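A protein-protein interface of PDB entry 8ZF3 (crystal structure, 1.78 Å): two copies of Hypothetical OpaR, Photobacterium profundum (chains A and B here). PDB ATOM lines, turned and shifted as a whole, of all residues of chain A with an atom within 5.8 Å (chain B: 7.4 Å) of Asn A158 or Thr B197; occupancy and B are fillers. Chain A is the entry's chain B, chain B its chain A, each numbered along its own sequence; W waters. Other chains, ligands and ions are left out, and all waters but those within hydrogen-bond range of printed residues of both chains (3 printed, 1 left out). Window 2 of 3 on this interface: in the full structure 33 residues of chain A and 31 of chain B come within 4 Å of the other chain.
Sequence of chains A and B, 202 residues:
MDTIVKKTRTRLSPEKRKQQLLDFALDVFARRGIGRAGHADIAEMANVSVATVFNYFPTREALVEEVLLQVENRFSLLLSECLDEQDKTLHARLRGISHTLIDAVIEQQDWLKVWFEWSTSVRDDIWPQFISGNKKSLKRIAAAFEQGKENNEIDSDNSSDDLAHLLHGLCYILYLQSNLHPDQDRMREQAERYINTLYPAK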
ATOM      1  N   LYS A 149       4.134  13.172 -18.395  1.00  0.00           N
ATOM      2  CA  LYS A 149       5.492  12.939 -17.920  1.00  0.00           C
ATOM      3  C   LYS A 149       5.495  12.161 -16.610  1.00  0.00           C
ATOM      4  O   LYS A 149       6.427  11.388 -16.354  1.00  0.00           O
ATOM      5  CB  LYS A 149       6.230  14.272 -17.765  1.00  0.00           C
ATOM      6  CG  LYS A 149       6.332  15.082 -19.048  1.00  0.00           C
ATOM      7  CD  LYS A 149       7.471  16.086 -18.957  1.00  0.00           C
ATOM      8  CE  LYS A 149       6.970  17.498 -18.797  1.00  0.00           C
ATOM      9  NZ  LYS A 149       8.042  18.391 -18.274  1.00  0.00           N
ATOM     10  N   ASP A 155       8.927  11.495 -22.803  1.00  0.00           N
ATOM     11  CA  ASP A 155      10.151  11.932 -22.145  1.00  0.00           C
ATOM     12  C   ASP A 155       9.865  13.076 -21.177  1.00  0.00           C
ATOM     13  O   ASP A 155       8.989  13.915 -21.412  1.00  0.00           O
ATOM     14  CB  ASP A 155      11.161  12.385 -23.194  1.00  0.00           C
ATOM     15  CG  ASP A 155      11.562  11.269 -24.130  1.00  0.00           C
ATOM     16  OD1 ASP A 155      12.144  11.574 -25.191  1.00  0.00           O
ATOM     17  OD2 ASP A 155      11.328  10.088 -23.793  1.00  0.00           O
ATOM     18  N   SER A 156      10.620  13.108 -20.075  1.00  0.00           N
ATOM     19  CA  SER A 156      10.562  14.215 -19.128  1.00  0.00           C
ATOM     20  C   SER A 156      11.513  15.345 -19.512  1.00  0.00           C
ATOM     21  O   SER A 156      11.680  16.295 -18.739  1.00  0.00           O
ATOM     22  CB  SER A 156      10.881  13.723 -17.711  1.00  0.00           C
ATOM     23  OG  SER A 156      12.073  12.936 -17.663  1.00  0.00           O
ATOM     24  N   ASP A 157      12.106  15.260 -20.705  1.00  0.00           N
ATOM     25  CA  ASP A 157      13.227  16.090 -21.122  1.00  0.00           C
ATOM     26  C   ASP A 157      12.827  17.509 -21.495  1.00  0.00           C
ATOM     27  O   ASP A 157      13.701  18.375 -21.617  1.00  0.00           O
ATOM     28  CB  ASP A 157      13.908  15.441 -22.325  1.00  0.00           C
ATOM     29  CG  ASP A 157      15.386  15.310 -22.145  1.00  0.00           C
ATOM     30  OD1 ASP A 157      15.904  15.793 -21.112  1.00  0.00           O
ATOM     31  OD2 ASP A 157      16.033  14.733 -23.045  1.00  0.00           O
ATOM     32  N   ASN A 158      11.538  17.760 -21.696  1.00  0.00           N
ATOM     33  CA  ASN A 158      11.064  19.026 -22.229  1.00  0.00           C
ATOM     34  C   ASN A 158      10.005  19.597 -21.298  1.00  0.00           C
ATOM     35  O   ASN A 158       9.128  18.866 -20.825  1.00  0.00           O
ATOM     36  CB  ASN A 158      10.503  18.841 -23.653  1.00  0.00           C
ATOM     37  CG  ASN A 158      11.493  18.158 -24.596  1.00  0.00           C
ATOM     38  OD1 ASN A 158      12.590  18.668 -24.847  1.00  0.00           O
ATOM     39  ND2 ASN A 158      11.107  16.990 -25.114  1.00  0.00           N
ATOM     40  N   SER A 159      10.080  20.908 -21.057  1.00  0.00           N
ATOM     41  CA  SER A 159       9.188  21.554 -20.104  1.00  0.00           C
ATOM     42  C   SER A 159       7.751  21.481 -20.599  1.00  0.00           C
ATOM     43  O   SER A 159       7.483  21.543 -21.802  1.00  0.00           O
ATOM     44  CB  SER A 159       9.594  23.012 -19.876  1.00  0.00           C
ATOM     45  OG  SER A 159       9.077  23.860 -20.885  1.00  0.00           O
ATOM     46  N   SER A 160       6.821  21.315 -19.663  1.00  0.00           N
ATOM     47  CA  SER A 160       5.421  21.198 -20.060  1.00  0.00           C
ATOM     48  C   SER A 160       4.933  22.448 -20.777  1.00  0.00           C
ATOM     49  O   SER A 160       4.127  22.347 -21.704  1.00  0.00           O
ATOM     50  CB  SER A 160       4.552  20.899 -18.841  1.00  0.00           C
ATOM     51  OG  SER A 160       4.749  19.557 -18.433  1.00  0.00           O
ATOM     52  N   ASP A 162       6.676  24.361 -22.813  1.00  0.00           N
ATOM     53  CA  ASP A 162       7.151  24.241 -24.194  1.00  0.00           C
ATOM     54  C   ASP A 162       6.327  23.235 -25.000  1.00  0.00           C
ATOM     55  O   ASP A 162       5.994  23.483 -26.166  1.00  0.00           O
ATOM     56  CB  ASP A 162       8.621  23.828 -24.216  1.00  0.00           C
ATOM     57  CG  ASP A 162       9.557  24.946 -23.814  1.00  0.00           C
ATOM     58  OD1 ASP A 162       9.120  26.113 -23.696  1.00  0.00           O
ATOM     59  OD2 ASP A 162      10.757  24.649 -23.612  1.00  0.00           O
ATOM     60  N   LEU A 163       6.025  22.078 -24.413  1.00  0.00           N
ATOM     61  CA  LEU A 163       5.200  21.091 -25.111  1.00  0.00           C
ATOM     62  C   LEU A 163       3.839  21.678 -25.467  1.00  0.00           C
ATOM     63  O   LEU A 163       3.303  21.417 -26.551  1.00  0.00           O
ATOM     64  CB  LEU A 163       5.046  19.829 -24.245  1.00  0.00           C
ATOM     65  CG  LEU A 163       6.363  19.110 -23.936  1.00  0.00           C
ATOM     66  CD1 LEU A 163       6.122  18.016 -22.913  1.00  0.00           C
ATOM     67  CD2 LEU A 163       6.905  18.500 -25.224  1.00  0.00           C
ATOM     68  N   LEU A 166       4.160  24.058 -28.392  1.00  0.00           N
ATOM     69  CA  LEU A 166       4.379  23.300 -29.620  1.00  0.00           C
ATOM     70  C   LEU A 166       3.096  22.658 -30.119  1.00  0.00           C
ATOM     71  O   LEU A 166       2.906  22.511 -31.334  1.00  0.00           O
ATOM     72  CB  LEU A 166       5.441  22.237 -29.397  1.00  0.00           C
ATOM     73  CG  LEU A 166       6.870  22.785 -29.339  1.00  0.00           C
ATOM     74  CD1 LEU A 166       7.747  21.712 -28.760  1.00  0.00           C
ATOM     75  CD2 LEU A 166       7.338  23.187 -30.720  1.00  0.00           C
ATOM     76  N   THR A 197       6.106  12.481 -34.163  1.00  0.00           N
ATOM     77  CA  THR A 197       7.344  13.232 -34.359  1.00  0.00           C
ATOM     78  C   THR A 197       7.616  14.147 -33.179  1.00  0.00           C
ATOM     79  O   THR A 197       8.743  14.228 -32.679  1.00  0.00           O
ATOM     80  CB  THR A 197       7.257  14.071 -35.640  1.00  0.00           C
ATOM     81  OG1 THR A 197       7.153  13.211 -36.784  1.00  0.00           O
ATOM     82  CG2 THR A 197       8.471  14.995 -35.767  1.00  0.00           C
ATOM     83  N   LEU A 198       6.587  14.857 -32.739  1.00  0.00           N
ATOM     84  CA  LEU A 198       6.771  15.857 -31.705  1.00  0.00           C
ATOM     85  C   LEU A 198       6.724  15.214 -30.323  1.00  0.00           C
ATOM     86  O   LEU A 198       7.485  15.596 -29.429  1.00  0.00           O
ATOM     87  CB  LEU A 198       5.705  16.934 -31.882  1.00  0.00           C
ATOM     88  CG  LEU A 198       5.729  18.237 -31.099  1.00  0.00           C
ATOM     89  CD1 LEU A 198       7.111  18.865 -31.133  1.00  0.00           C
ATOM     90  CD2 LEU A 198       4.723  19.140 -31.746  1.00  0.00           C
ATOM     91  N   ALA B 191      13.660  29.783 -28.673  1.00  0.00           N
ATOM     92  CA  ALA B 191      13.748  29.090 -29.958  1.00  0.00           C
ATOM     93  C   ALA B 191      14.628  27.844 -29.863  1.00  0.00           C
ATOM     94  O   ALA B 191      14.285  26.785 -30.405  1.00  0.00           O
ATOM     95  CB  ALA B 191      14.288  30.040 -31.025  1.00  0.00           C
ATOM     96  N   GLU B 192      15.769  27.957 -29.188  1.00  0.00           N
ATOM     97  CA  GLU B 192      16.662  26.810 -29.034  1.00  0.00           C
ATOM     98  C   GLU B 192      15.964  25.637 -28.350  1.00  0.00           C
ATOM     99  O   GLU B 192      16.103  24.483 -28.779  1.00  0.00           O
ATOM    100  CB  GLU B 192      17.907  27.234 -28.260  1.00  0.00           C
ATOM    101  CG  GLU B 192      18.966  26.168 -28.193  1.00  0.00           C
ATOM    102  CD  GLU B 192      20.195  26.634 -27.455  1.00  0.00           C
ATOM    103  OE1 GLU B 192      21.306  26.302 -27.919  1.00  0.00           O
ATOM    104  OE2 GLU B 192      20.062  27.362 -26.438  1.00  0.00           O
ATOM    105  N   ARG B 193      15.181  25.919 -27.304  1.00  0.00           N
ATOM    106  CA  ARG B 193      14.454  24.855 -26.617  1.00  0.00           C
ATOM    107  C   ARG B 193      13.421  24.212 -27.535  1.00  0.00           C
ATOM    108  O   ARG B 193      13.286  22.981 -27.554  1.00  0.00           O
ATOM    109  CB  ARG B 193      13.781  25.401 -25.359  1.00  0.00           C
ATOM    110  CG  ARG B 193      14.749  25.701 -24.208  1.00  0.00           C
ATOM    111  CD  ARG B 193      14.070  25.578 -22.843  1.00  0.00           C
ATOM    112  NE  ARG B 193      12.808  26.311 -22.804  1.00  0.00           N
ATOM    113  CZ  ARG B 193      12.694  27.629 -22.693  1.00  0.00           C
ATOM    114  NH1 ARG B 193      13.757  28.411 -22.592  1.00  0.00           N
ATOM    115  NH2 ARG B 193      11.481  28.177 -22.688  1.00  0.00           N
ATOM    116  N   TYR B 194      12.691  25.019 -28.302  1.00  0.00           N
ATOM    117  CA  TYR B 194      11.740  24.462 -29.263  1.00  0.00           C
ATOM    118  C   TYR B 194      12.447  23.553 -30.255  1.00  0.00           C
ATOM    119  O   TYR B 194      11.978  22.450 -30.547  1.00  0.00           O
ATOM    120  CB  TYR B 194      11.039  25.580 -30.024  1.00  0.00           C
ATOM    121  CG  TYR B 194      10.007  26.344 -29.251  1.00  0.00           C
ATOM    122  CD1 TYR B 194       9.318  25.762 -28.199  1.00  0.00           C
ATOM    123  CD2 TYR B 194       9.706  27.654 -29.592  1.00  0.00           C
ATOM    124  CE1 TYR B 194       8.359  26.473 -27.502  1.00  0.00           C
ATOM    125  CE2 TYR B 194       8.759  28.374 -28.909  1.00  0.00           C
ATOM    126  CZ  TYR B 194       8.087  27.781 -27.865  1.00  0.00           C
ATOM    127  OH  TYR B 194       7.140  28.509 -27.182  1.00  0.00           O
ATOM    128  N   ILE B 195      13.548  24.035 -30.834  1.00  0.00           N
ATOM    129  CA  ILE B 195      14.286  23.243 -31.815  1.00  0.00           C
ATOM    130  C   ILE B 195      14.775  21.931 -31.206  1.00  0.00           C
ATOM    131  O   ILE B 195      14.693  20.878 -31.844  1.00  0.00           O
ATOM    132  CB  ILE B 195      15.441  24.073 -32.416  1.00  0.00           C
ATOM    133  CG1 ILE B 195      14.889  25.177 -33.322  1.00  0.00           C
ATOM    134  CG2 ILE B 195      16.412  23.204 -33.203  1.00  0.00           C
ATOM    135  CD1 ILE B 195      15.905  26.290 -33.600  1.00  0.00           C
ATOM    136  N   ASN B 196      15.275  21.963 -29.965  1.00  0.00           N
ATOM    137  CA  ASN B 196      15.778  20.736 -29.340  1.00  0.00           C
ATOM    138  C   ASN B 196      14.664  19.730 -29.084  1.00  0.00           C
ATOM    139  O   ASN B 196      14.905  18.518 -29.123  1.00  0.00           O
ATOM    140  CB  ASN B 196      16.487  21.043 -28.021  1.00  0.00           C
ATOM    141  CG  ASN B 196      17.762  21.819 -28.213  1.00  0.00           C
ATOM    142  OD1 ASN B 196      18.361  21.806 -29.290  1.00  0.00           O
ATOM    143  ND2 ASN B 196      18.197  22.497 -27.159  1.00  0.00           N
ATOM    144  N   THR B 197      13.452  20.208 -28.807  1.00  0.00           N
ATOM    145  CA  THR B 197      12.320  19.319 -28.563  1.00  0.00           C
ATOM    146  C   THR B 197      11.805  18.699 -29.857  1.00  0.00           C
ATOM    147  O   THR B 197      11.522  17.493 -29.913  1.00  0.00           O
ATOM    148  CB  THR B 197      11.206  20.097 -27.864  1.00  0.00           C
ATOM    149  OG1 THR B 197      11.727  20.667 -26.658  1.00  0.00           O
ATOM    150  CG2 THR B 197      10.017  19.188 -27.551  1.00  0.00           C
ATOM    151  N   LEU B 198      11.669  19.526 -30.897  1.00  0.00           N
ATOM    152  CA  LEU B 198      11.142  19.124 -32.196  1.00  0.00           C
ATOM    153  C   LEU B 198      12.157  18.326 -33.005  1.00  0.00           C
ATOM    154  O   LEU B 198      11.795  17.367 -33.703  1.00  0.00           O
ATOM    155  CB  LEU B 198      10.729  20.381 -32.959  1.00  0.00           C
ATOM    156  CG  LEU B 198       9.936  20.314 -34.253  1.00  0.00           C
ATOM    157  CD1 LEU B 198       8.838  19.265 -34.166  1.00  0.00           C
ATOM    158  CD2 LEU B 198       9.364  21.694 -34.531  1.00  0.00           C
ATOM    159  N   TYR B 199      13.433  18.708 -32.913  1.00  0.00           N
ATOM    160  CA  TYR B 199      14.498  18.138 -33.741  1.00  0.00           C
ATOM    161  C   TYR B 199      15.647  17.661 -32.864  1.00  0.00           C
ATOM    162  O   TYR B 199      16.725  18.281 -32.823  1.00  0.00           O
ATOM    163  CB  TYR B 199      14.984  19.166 -34.764  1.00  0.00           C
ATOM    164  CG  TYR B 199      13.853  19.753 -35.574  1.00  0.00           C
ATOM    165  CD1 TYR B 199      13.090  18.954 -36.413  1.00  0.00           C
ATOM    166  CD2 TYR B 199      13.554  21.112 -35.511  1.00  0.00           C
ATOM    167  CE1 TYR B 199      12.038  19.482 -37.162  1.00  0.00           C
ATOM    168  CE2 TYR B 199      12.527  21.647 -36.250  1.00  0.00           C
ATOM    169  CZ  TYR B 199      11.768  20.829 -37.074  1.00  0.00           C
ATOM    170  OH  TYR B 199      10.743  21.365 -37.822  1.00  0.00           O
ATOM    171  N   PRO B 200      15.462  16.538 -32.173  1.00  0.00           N
ATOM    172  CA  PRO B 200      16.515  16.052 -31.267  1.00  0.00           C
ATOM    173  C   PRO B 200      17.782  15.703 -32.033  1.00  0.00           C
ATOM    174  O   PRO B 200      17.739  15.182 -33.152  1.00  0.00           O
ATOM    175  CB  PRO B 200      15.900  14.808 -30.610  1.00  0.00           C
ATOM    176  CG  PRO B 200      14.486  14.688 -31.115  1.00  0.00           C
ATOM    177  CD  PRO B 200      14.187  15.797 -32.057  1.00  0.00           C
ATOM    178  N   ALA B 201      18.920  15.993 -31.410  1.00  0.00           N
ATOM    179  CA  ALA B 201      20.204  15.768 -32.050  1.00  0.00           C
ATOM    180  C   ALA B 201      20.480  14.279 -32.236  1.00  0.00           C
ATOM    181  O   ALA B 201      19.988  13.426 -31.492  1.00  0.00           O
ATOM    182  CB  ALA B 201      21.325  16.397 -31.220  1.00  0.00           C
HETATM  183  O   HOH W   1      10.822  15.080 -31.034  1.00  0.00           O
HETATM  184  O   HOH W   2      13.106  16.114 -27.568  1.00  0.00           O
HETATM  185  O   HOH W   3       7.119  27.860 -23.908  1.00  0.00           O
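OD2 of Asp A162 lies within salt-bridge range of NE of Arg B193 (2.8 Å).
OG1 of Thr B197 sits at hydrogen-bond distance from OD1 of Asn A158 (2.8 Å).
O of Arg B193 is in hydrogen-bond range of OG1 of Thr B197 (2.9 Å).
NZ of Lys A149 is in hydrogen-bond range of O of Asn A158 (2.8 Å).
The backbone NH (N) of Asp A162 is in hydrogen-bond range of the side-chain hydroxyl (OG) of Ser A159 (3.1 Å).
Among the printed residues, pairs that only touch across the chains: Leu A198 with Leu B198, Leu A166 with Thr B197, Asp A162 with Tyr B194 and Leu A163 with Thr B197.
Asn A158 touches just one residue of chain B: Thr B197.
Of the printed residues of chain B, Leu A166 touches Thr B197.
Of the printed residues of chain B, Leu A198 touches Leu B198 (3.5 Å).
Of the printed residues of chain A, Tyr B194 touches Asp A162.
Thr B197 touches just these residues of chain A: Asn A158 (2.8 Å), Leu A163 (3.9 Å) and Leu A166 (3.6 Å).
The nearest residue of chain B that does not touch Asn A158 is Asn B196 (4.8 Å).
The nearest residue of chain A that does not touch Thr B197 is Leu A198 (4.5 Å).
Of the 12 printed residues of chain A, 5 touch a printed residue of chain B.
Hydrophobic or aromatic side chains of chain B within 4 Å of the printed part of chain A: Tyr B194 and Leu B198.
Among the printed residues, Asp or Glu carboxylates within 4 Å of a Lys or Arg side-chain nitrogen of the other chain: Asp A162 with Arg B193.
Leu B198 touches its own counterpart, Leu A198.
Positions printed for both chains: 197 and 198.
Of the 6 pairs that touch across the chains among the printed residues, 1 has its exchanged pair printed and touching as well.
Water W3 lies within hydrogen-bond range of the side-chain carboxylate (OD1) of Asp A162 (2.7 Å) and the side-chain hydroxyl (OH) of Tyr B194 (3.3 Å).
Water W1 lies within hydrogen-bond range of the backbone carbonyl oxygen of Thr B197 and the backbone carbonyl oxygen of Thr A197.
Water W2 lies within hydrogen-bond range of the backbone carbonyl oxygen (O) of Thr B197 (3.1 Å), the side-chain amide nitrogen (ND2) of Asn A158 (3.3 Å) and the backbone carbonyl oxygen (O) of Asn B196 (3.4 Å).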
